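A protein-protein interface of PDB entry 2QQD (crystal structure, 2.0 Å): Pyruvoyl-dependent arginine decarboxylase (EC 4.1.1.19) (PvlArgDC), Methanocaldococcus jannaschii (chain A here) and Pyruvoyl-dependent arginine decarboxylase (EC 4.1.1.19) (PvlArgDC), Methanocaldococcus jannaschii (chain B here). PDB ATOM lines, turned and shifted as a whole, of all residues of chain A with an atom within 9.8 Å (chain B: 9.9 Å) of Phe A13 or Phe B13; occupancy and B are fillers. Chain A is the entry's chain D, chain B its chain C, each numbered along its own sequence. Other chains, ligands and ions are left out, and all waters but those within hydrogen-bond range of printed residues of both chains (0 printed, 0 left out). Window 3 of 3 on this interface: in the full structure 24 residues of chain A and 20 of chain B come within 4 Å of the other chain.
Hydrophobic or aromatic side chains of chain A within 4 Å of the printed part of chain B: His A10 and Phe A13.
Of the 12 printed residues of chain B, 6 touch a printed residue of chain A.
Printed residues of chain B that touch a printed residue of chain A: Tyr B12, Phe B13, Lys B14, Leu B15, Trp B164 and Tyr B165.
Hydrophobic or aromatic side chains of chain B within 4 Å of the printed part of chain A: Phe B13, Leu B15, Trp B164 and Tyr B165.
The backbone carbonyl oxygen (O) of Trp B164 sits at hydrogen-bond distance from the backbone NH (N) of Asn B17, 2.9 Å away.
The backbone NH (N) of Leu A9 sits at hydrogen-bond distance from the side-chain amide oxygen (OD1) of Asn A7, 3.0 Å away.
OH of Tyr B165 lies within hydrogen-bond range of O of Lys B14, at 2.7 Å.
Phe A13 touches one residue of chain B.
Phe B13 touches six residues of chain A.
Ala A11 touches just one residue of chain B: Phe B13.
Of the printed residues of chain A, Tyr B165 touches Asn A7 (2.7 Å) and His A10 (3.6 Å).
Of the printed residues of chain A, Lys B14 touches Glu A5 and Asn A7.
Of the printed residues of chain A, Trp B164 touches His A10 (3.8 Å).
Of the printed residues of chain B, His A10 touches Tyr B12 (2.5 Å), Phe B13 (3.4 Å), Trp B164 (3.8 Å) and Tyr B165 (3.6 Å).
Pro B8 touches none of the printed residues of chain A.
Asn B17 touches none of the printed residues of chain A.
The nearest residue of chain B that does not touch Phe A13 is His B10 (7.1 Å).
Among the printed residues, pairs that only touch across the chains: Glu A5 with Phe B13, Glu A5 with Lys B14, Ile A6 with Phe B13, Ile A6 with Leu B15, Asn A7 with Lys B14, His A10 with Phe B13, His A10 with Trp B164, His A10 with Tyr B165, Ala A11 with Phe B13 and Phe A13 with Phe B13.
The side-chain amide nitrogen of Asn A7 lies within hydrogen-bond range of the side-chain hydroxyl of Tyr B165, 2.7 Å away.
OE1 of Glu A5 lies within hydrogen-bond range of N of Leu B15 (3.0 Å).
The backbone carbonyl oxygen (O) of Tyr B12 sits at hydrogen-bond distance from a ring nitrogen (ND1) of His A10 (2.5 Å).
O of Phe B13 lies within hydrogen-bond range of N of Asn A7 (2.9 Å).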
ATOM      1  N   ALA A   4      12.906 -12.958   7.850  1.00  0.00           N
ATOM      2  CA  ALA A   4      12.278 -12.735   6.513  1.00  0.00           C
ATOM      3  C   ALA A   4      12.172 -14.037   5.709  1.00  0.00           C
ATOM      4  O   ALA A   4      11.541 -14.080   4.651  1.00  0.00           O
ATOM      5  CB  ALA A   4      13.086 -11.710   5.735  1.00  0.00           C
ATOM      6  N   GLU A   5      12.794 -15.096   6.210  1.00  0.00           N
ATOM      7  CA  GLU A   5      12.761 -16.387   5.531  1.00  0.00           C
ATOM      8  C   GLU A   5      11.882 -17.385   6.268  1.00  0.00           C
ATOM      9  O   GLU A   5      11.644 -17.252   7.467  1.00  0.00           O
ATOM     10  CB  GLU A   5      14.172 -16.967   5.425  1.00  0.00           C
ATOM     11  CG  GLU A   5      15.060 -16.314   4.382  1.00  0.00           C
ATOM     12  CD  GLU A   5      16.495 -16.819   4.456  1.00  0.00           C
ATOM     13  OE1 GLU A   5      16.690 -18.014   4.761  1.00  0.00           O
ATOM     14  OE2 GLU A   5      17.427 -16.022   4.205  1.00  0.00           O
ATOM     15  N   ILE A   6      11.395 -18.385   5.544  1.00  0.00           N
ATOM     16  CA  ILE A   6      10.580 -19.420   6.162  1.00  0.00           C
ATOM     17  C   ILE A   6      10.647 -20.733   5.398  1.00  0.00           C
ATOM     18  O   ILE A   6      10.688 -20.755   4.169  1.00  0.00           O
ATOM     19  CB  ILE A   6       9.089 -19.006   6.278  1.00  0.00           C
ATOM     20  CG1 ILE A   6       8.325 -20.072   7.075  1.00  0.00           C
ATOM     21  CG2 ILE A   6       8.468 -18.854   4.888  1.00  0.00           C
ATOM     22  CD1 ILE A   6       6.881 -19.710   7.385  1.00  0.00           C
ATOM     23  N   ASN A   7      10.690 -21.827   6.144  1.00  0.00           N
ATOM     24  CA  ASN A   7      10.688 -23.154   5.550  1.00  0.00           C
ATOM     25  C   ASN A   7       9.355 -23.735   6.017  1.00  0.00           C
ATOM     26  O   ASN A   7       9.238 -24.206   7.153  1.00  0.00           O
ATOM     27  CB  ASN A   7      11.846 -24.008   6.081  1.00  0.00           C
ATOM     28  CG  ASN A   7      11.854 -25.403   5.479  1.00  0.00           C
ATOM     29  OD1 ASN A   7      10.859 -25.837   4.894  1.00  0.00           O
ATOM     30  ND2 ASN A   7      12.964 -26.115   5.630  1.00  0.00           N
ATOM     31  N   PRO A   8       8.324 -23.687   5.152  1.00  0.00           N
ATOM     32  CA  PRO A   8       6.993 -24.208   5.488  1.00  0.00           C
ATOM     33  C   PRO A   8       6.986 -25.648   6.018  1.00  0.00           C
ATOM     34  O   PRO A   8       6.058 -26.051   6.715  1.00  0.00           O
ATOM     35  CB  PRO A   8       6.226 -24.077   4.170  1.00  0.00           C
ATOM     36  CG  PRO A   8       6.882 -22.910   3.509  1.00  0.00           C
ATOM     37  CD  PRO A   8       8.348 -23.162   3.776  1.00  0.00           C
ATOM     38  N   LEU A   9       8.011 -26.423   5.681  1.00  0.00           N
ATOM     39  CA  LEU A   9       8.104 -27.807   6.142  1.00  0.00           C
ATOM     40  C   LEU A   9       8.445 -27.866   7.633  1.00  0.00           C
ATOM     41  O   LEU A   9       8.142 -28.849   8.310  1.00  0.00           O
ATOM     42  CB  LEU A   9       9.177 -28.556   5.345  1.00  0.00           C
ATOM     43  CG  LEU A   9       8.948 -28.674   3.835  1.00  0.00           C
ATOM     44  CD1 LEU A   9      10.169 -29.287   3.167  1.00  0.00           C
ATOM     45  CD2 LEU A   9       7.712 -29.522   3.571  1.00  0.00           C
ATOM     46  N   HIS A  10       9.085 -26.815   8.136  1.00  0.00           N
ATOM     47  CA  HIS A  10       9.463 -26.759   9.542  1.00  0.00           C
ATOM     48  C   HIS A  10       8.514 -25.875  10.350  1.00  0.00           C
ATOM     49  O   HIS A  10       8.141 -26.221  11.470  1.00  0.00           O
ATOM     50  CB  HIS A  10      10.906 -26.270   9.667  1.00  0.00           C
ATOM     51  CG  HIS A  10      11.915 -27.260   9.172  1.00  0.00           C
ATOM     52  ND1 HIS A  10      13.251 -26.956   9.027  1.00  0.00           N
ATOM     53  CD2 HIS A  10      11.784 -28.559   8.808  1.00  0.00           C
ATOM     54  CE1 HIS A  10      13.900 -28.024   8.597  1.00  0.00           C
ATOM     55  NE2 HIS A  10      13.034 -29.009   8.456  1.00  0.00           N
ATOM     56  N   ALA A  11       8.122 -24.741   9.776  1.00  0.00           N
ATOM     57  CA  ALA A  11       7.191 -23.835  10.435  1.00  0.00           C
ATOM     58  C   ALA A  11       5.758 -24.277  10.096  1.00  0.00           C
ATOM     59  O   ALA A  11       5.018 -23.561   9.417  1.00  0.00           O
ATOM     60  CB  ALA A  11       7.434 -22.408   9.963  1.00  0.00           C
ATOM     61  N   TYR A  12       5.380 -25.460  10.578  1.00  0.00           N
ATOM     62  CA  TYR A  12       4.054 -26.026  10.334  1.00  0.00           C
ATOM     63  C   TYR A  12       2.932 -25.212  10.992  1.00  0.00           C
ATOM     64  O   TYR A  12       1.775 -25.287  10.578  1.00  0.00           O
ATOM     65  CB  TYR A  12       4.012 -27.469  10.852  1.00  0.00           C
ATOM     66  CG  TYR A  12       4.121 -27.576  12.355  1.00  0.00           C
ATOM     67  CD1 TYR A  12       2.987 -27.472  13.160  1.00  0.00           C
ATOM     68  CD2 TYR A  12       5.365 -27.732  12.981  1.00  0.00           C
ATOM     69  CE1 TYR A  12       3.078 -27.518  14.545  1.00  0.00           C
ATOM     70  CE2 TYR A  12       5.464 -27.774  14.374  1.00  0.00           C
ATOM     71  CZ  TYR A  12       4.313 -27.666  15.146  1.00  0.00           C
ATOM     72  OH  TYR A  12       4.385 -27.707  16.520  1.00  0.00           O
ATOM     73  N   PHE A  13       3.285 -24.438  12.018  1.00  0.00           N
ATOM     74  CA  PHE A  13       2.318 -23.624  12.751  1.00  0.00           C
ATOM     75  C   PHE A  13       2.064 -22.261  12.102  1.00  0.00           C
ATOM     76  O   PHE A  13       1.189 -21.512  12.532  1.00  0.00           O
ATOM     77  CB  PHE A  13       2.805 -23.442  14.197  1.00  0.00           C
ATOM     78  CG  PHE A  13       4.238 -22.992  14.293  1.00  0.00           C
ATOM     79  CD1 PHE A  13       4.576 -21.653  14.120  1.00  0.00           C
ATOM     80  CD2 PHE A  13       5.254 -23.916  14.501  1.00  0.00           C
ATOM     81  CE1 PHE A  13       5.902 -21.242  14.149  1.00  0.00           C
ATOM     82  CE2 PHE A  13       6.593 -23.516  14.532  1.00  0.00           C
ATOM     83  CZ  PHE A  13       6.917 -22.177  14.355  1.00  0.00           C
ATOM     84  N   LYS A  14       2.828 -21.931  11.068  1.00  0.00           N
ATOM     85  CA  LYS A  14       2.643 -20.658  10.381  1.00  0.00           C
ATOM     86  C   LYS A  14       2.090 -20.972   8.996  1.00  0.00           C
ATOM     87  O   LYS A  14       2.822 -21.396   8.104  1.00  0.00           O
ATOM     88  CB  LYS A  14       3.975 -19.904  10.273  1.00  0.00           C
ATOM     89  CG  LYS A  14       3.844 -18.458   9.809  1.00  0.00           C
ATOM     90  CD  LYS A  14       2.890 -17.672  10.714  1.00  0.00           C
ATOM     91  CE  LYS A  14       3.067 -16.163  10.566  1.00  0.00           C
ATOM     92  NZ  LYS A  14       2.757 -15.643   9.204  1.00  0.00           N
ATOM     93  N   LEU A  15       0.789 -20.779   8.827  1.00  0.00           N
ATOM     94  CA  LEU A  15       0.147 -21.078   7.555  1.00  0.00           C
ATOM     95  C   LEU A  15       0.117 -19.908   6.588  1.00  0.00           C
ATOM     96  O   LEU A  15       0.034 -18.752   6.999  1.00  0.00           O
ATOM     97  CB  LEU A  15      -1.283 -21.571   7.794  1.00  0.00           C
ATOM     98  CG  LEU A  15      -1.447 -22.973   8.396  1.00  0.00           C
ATOM     99  CD1 LEU A  15      -0.687 -23.081   9.707  1.00  0.00           C
ATOM    100  CD2 LEU A  15      -2.932 -23.248   8.612  1.00  0.00           C
ATOM    101  N   PRO A  16       0.191 -20.201   5.280  1.00  0.00           N
ATOM    102  CA  PRO A  16       0.163 -19.168   4.239  1.00  0.00           C
ATOM    103  C   PRO A  16      -1.145 -18.393   4.378  1.00  0.00           C
ATOM    104  O   PRO A  16      -2.139 -18.942   4.866  1.00  0.00           O
ATOM    105  CB  PRO A  16       0.202 -19.979   2.942  1.00  0.00           C
ATOM    106  CG  PRO A  16       0.944 -21.240   3.347  1.00  0.00           C
ATOM    107  CD  PRO A  16       0.339 -21.546   4.692  1.00  0.00           C
ATOM    108  N   PRO B   8      22.257 -16.315  16.078  1.00  0.00           N
ATOM    109  CA  PRO B   8      21.302 -16.626  14.985  1.00  0.00           C
ATOM    110  C   PRO B   8      20.373 -17.734  15.459  1.00  0.00           C
ATOM    111  O   PRO B   8      20.732 -18.910  15.442  1.00  0.00           O
ATOM    112  CB  PRO B   8      22.128 -17.085  13.797  1.00  0.00           C
ATOM    113  CG  PRO B   8      23.327 -17.716  14.508  1.00  0.00           C
ATOM    114  CD  PRO B   8      23.606 -16.786  15.712  1.00  0.00           C
ATOM    115  N   LEU B   9      19.180 -17.351  15.896  1.00  0.00           N
ATOM    116  CA  LEU B   9      18.216 -18.321  16.395  1.00  0.00           C
ATOM    117  C   LEU B   9      17.171 -18.669  15.341  1.00  0.00           C
ATOM    118  O   LEU B   9      17.045 -17.975  14.335  1.00  0.00           O
ATOM    119  CB  LEU B   9      17.539 -17.768  17.654  1.00  0.00           C
ATOM    120  CG  LEU B   9      18.490 -17.552  18.836  1.00  0.00           C
ATOM    121  CD1 LEU B   9      17.757 -16.892  19.988  1.00  0.00           C
ATOM    122  CD2 LEU B   9      19.067 -18.892  19.271  1.00  0.00           C
ATOM    123  N   HIS B  10      16.426 -19.744  15.575  1.00  0.00           N
ATOM    124  CA  HIS B  10      15.389 -20.172  14.638  1.00  0.00           C
ATOM    125  C   HIS B  10      15.957 -20.441  13.248  1.00  0.00           C
ATOM    126  O   HIS B  10      15.253 -20.296  12.250  1.00  0.00           O
ATOM    127  CB  HIS B  10      14.303 -19.097  14.532  1.00  0.00           C
ATOM    128  CG  HIS B  10      13.476 -18.944  15.770  1.00  0.00           C
ATOM    129  ND1 HIS B  10      12.801 -17.780  16.073  1.00  0.00           N
ATOM    130  CD2 HIS B  10      13.205 -19.808  16.775  1.00  0.00           C
ATOM    131  CE1 HIS B  10      12.153 -17.936  17.214  1.00  0.00           C
ATOM    132  NE2 HIS B  10      12.381 -19.157  17.660  1.00  0.00           N
ATOM    133  N   ALA B  11      17.227 -20.829  13.188  1.00  0.00           N
ATOM    134  CA  ALA B  11      17.874 -21.111  11.908  1.00  0.00           C
ATOM    135  C   ALA B  11      17.112 -22.167  11.104  1.00  0.00           C
ATOM    136  O   ALA B  11      16.961 -22.039   9.892  1.00  0.00           O
ATOM    137  CB  ALA B  11      19.316 -21.569  12.135  1.00  0.00           C
ATOM    138  N   TYR B  12      16.625 -23.200  11.782  1.00  0.00           N
ATOM    139  CA  TYR B  12      15.899 -24.272  11.108  1.00  0.00           C
ATOM    140  C   TYR B  12      14.533 -23.870  10.559  1.00  0.00           C
ATOM    141  O   TYR B  12      13.879 -24.651   9.866  1.00  0.00           O
ATOM    142  CB  TYR B  12      15.767 -25.476  12.046  1.00  0.00           C
ATOM    143  CG  TYR B  12      16.985 -26.372  12.026  1.00  0.00           C
ATOM    144  CD1 TYR B  12      17.091 -27.413  11.103  1.00  0.00           C
ATOM    145  CD2 TYR B  12      18.049 -26.157  12.901  1.00  0.00           C
ATOM    146  CE1 TYR B  12      18.221 -28.218  11.051  1.00  0.00           C
ATOM    147  CE2 TYR B  12      19.192 -26.956  12.852  1.00  0.00           C
ATOM    148  CZ  TYR B  12      19.269 -27.984  11.924  1.00  0.00           C
ATOM    149  OH  TYR B  12      20.394 -28.772  11.861  1.00  0.00           O
ATOM    150  N   PHE B  13      14.102 -22.651  10.859  1.00  0.00           N
ATOM    151  CA  PHE B  13      12.824 -22.181  10.367  1.00  0.00           C
ATOM    152  C   PHE B  13      13.003 -21.284   9.151  1.00  0.00           C
ATOM    153  O   PHE B  13      12.027 -20.830   8.553  1.00  0.00           O
ATOM    154  CB  PHE B  13      12.065 -21.451  11.470  1.00  0.00           C
ATOM    155  CG  PHE B  13      11.577 -22.359  12.558  1.00  0.00           C
ATOM    156  CD1 PHE B  13      10.681 -23.384  12.269  1.00  0.00           C
ATOM    157  CD2 PHE B  13      12.020 -22.199  13.871  1.00  0.00           C
ATOM    158  CE1 PHE B  13      10.225 -24.243  13.270  1.00  0.00           C
ATOM    159  CE2 PHE B  13      11.573 -23.053  14.885  1.00  0.00           C
ATOM    160  CZ  PHE B  13      10.671 -24.077  14.582  1.00  0.00           C
ATOM    161  N   LYS B  14      14.258 -21.036   8.792  1.00  0.00           N
ATOM    162  CA  LYS B  14      14.580 -20.208   7.635  1.00  0.00           C
ATOM    163  C   LYS B  14      14.920 -21.159   6.488  1.00  0.00           C
ATOM    164  O   LYS B  14      14.730 -22.363   6.603  1.00  0.00           O
ATOM    165  CB  LYS B  14      15.784 -19.309   7.938  1.00  0.00           C
ATOM    166  CG  LYS B  14      15.647 -18.507   9.229  1.00  0.00           C
ATOM    167  CD  LYS B  14      16.858 -17.602   9.461  1.00  0.00           C
ATOM    168  CE  LYS B  14      16.828 -16.980  10.853  1.00  0.00           C
ATOM    169  NZ  LYS B  14      15.542 -16.266  11.129  1.00  0.00           N
ATOM    170  N   LEU B  15      15.426 -20.615   5.393  1.00  0.00           N
ATOM    171  CA  LEU B  15      15.793 -21.422   4.233  1.00  0.00           C
ATOM    172  C   LEU B  15      17.038 -22.276   4.453  1.00  0.00           C
ATOM    173  O   LEU B  15      17.944 -21.909   5.207  1.00  0.00           O
ATOM    174  CB  LEU B  15      16.028 -20.513   3.016  1.00  0.00           C
ATOM    175  CG  LEU B  15      15.009 -20.493   1.869  1.00  0.00           C
ATOM    176  CD1 LEU B  15      13.589 -20.590   2.404  1.00  0.00           C
ATOM    177  CD2 LEU B  15      15.208 -19.218   1.038  1.00  0.00           C
ATOM    178  N   PRO B  16      17.097 -23.439   3.790  1.00  0.00           N
ATOM    179  CA  PRO B  16      18.267 -24.309   3.933  1.00  0.00           C
ATOM    180  C   PRO B  16      19.479 -23.511   3.432  1.00  0.00           C
ATOM    181  O   PRO B  16      19.336 -22.661   2.558  1.00  0.00           O
ATOM    182  CB  PRO B  16      17.941 -25.482   3.010  1.00  0.00           C
ATOM    183  CG  PRO B  16      16.419 -25.519   3.022  1.00  0.00           C
ATOM    184  CD  PRO B  16      16.061 -24.058   2.946  1.00  0.00           C
ATOM    185  N   ASN B  17      20.661 -23.759   3.986  1.00  0.00           N
ATOM    186  CA  ASN B  17      21.843 -23.038   3.527  1.00  0.00           C
ATOM    187  C   ASN B  17      22.928 -23.962   2.967  1.00  0.00           C
ATOM    188  O   ASN B  17      24.030 -23.512   2.643  1.00  0.00           O
ATOM    189  CB  ASN B  17      22.413 -22.157   4.644  1.00  0.00           C
ATOM    190  CG  ASN B  17      22.469 -22.872   5.963  1.00  0.00           C
ATOM    191  OD1 ASN B  17      22.856 -24.031   6.024  1.00  0.00           O
ATOM    192  ND2 ASN B  17      22.085 -22.185   7.032  1.00  0.00           N
ATOM    193  N   TRP B 164      19.920 -28.792   3.171  1.00  0.00           N
ATOM    194  CA  TRP B 164      19.802 -28.883   4.612  1.00  0.00           C
ATOM    195  C   TRP B 164      20.394 -27.653   5.287  1.00  0.00           C
ATOM    196  O   TRP B 164      20.478 -26.588   4.687  1.00  0.00           O
ATOM    197  CB  TRP B 164      20.456 -30.173   5.139  1.00  0.00           C
ATOM    198  CG  TRP B 164      19.946 -30.590   6.519  1.00  0.00           C
ATOM    199  CD1 TRP B 164      20.705 -30.905   7.615  1.00  0.00           C
ATOM    200  CD2 TRP B 164      18.574 -30.702   6.941  1.00  0.00           C
ATOM    201  NE1 TRP B 164      19.893 -31.200   8.692  1.00  0.00           N
ATOM    202  CE2 TRP B 164      18.585 -31.084   8.306  1.00  0.00           C
ATOM    203  CE3 TRP B 164      17.339 -30.517   6.302  1.00  0.00           C
ATOM    204  CZ2 TRP B 164      17.409 -31.279   9.040  1.00  0.00           C
ATOM    205  CZ3 TRP B 164      16.169 -30.712   7.036  1.00  0.00           C
ATOM    206  CH2 TRP B 164      16.216 -31.090   8.389  1.00  0.00           C
ATOM    207  N   TYR B 165      20.805 -27.806   6.538  1.00  0.00           N
ATOM    208  CA  TYR B 165      21.331 -26.682   7.288  1.00  0.00           C
ATOM    209  C   TYR B 165      22.727 -26.909   7.818  1.00  0.00           C
ATOM    210  O   TYR B 165      23.083 -28.014   8.222  1.00  0.00           O
ATOM    211  CB  TYR B 165      20.384 -26.374   8.443  1.00  0.00           C
ATOM    212  CG  TYR B 165      18.995 -26.018   7.971  1.00  0.00           C
ATOM    213  CD1 TYR B 165      18.556 -24.701   7.984  1.00  0.00           C
ATOM    214  CD2 TYR B 165      18.130 -26.998   7.471  1.00  0.00           C
ATOM    215  CE1 TYR B 165      17.299 -24.357   7.517  1.00  0.00           C
ATOM    216  CE2 TYR B 165      16.862 -26.662   6.995  1.00  0.00           C
ATOM    217  CZ  TYR B 165      16.457 -25.338   7.023  1.00  0.00           C
ATOM    218  OH  TYR B 165      15.217 -24.980   6.557  1.00  0.00           O
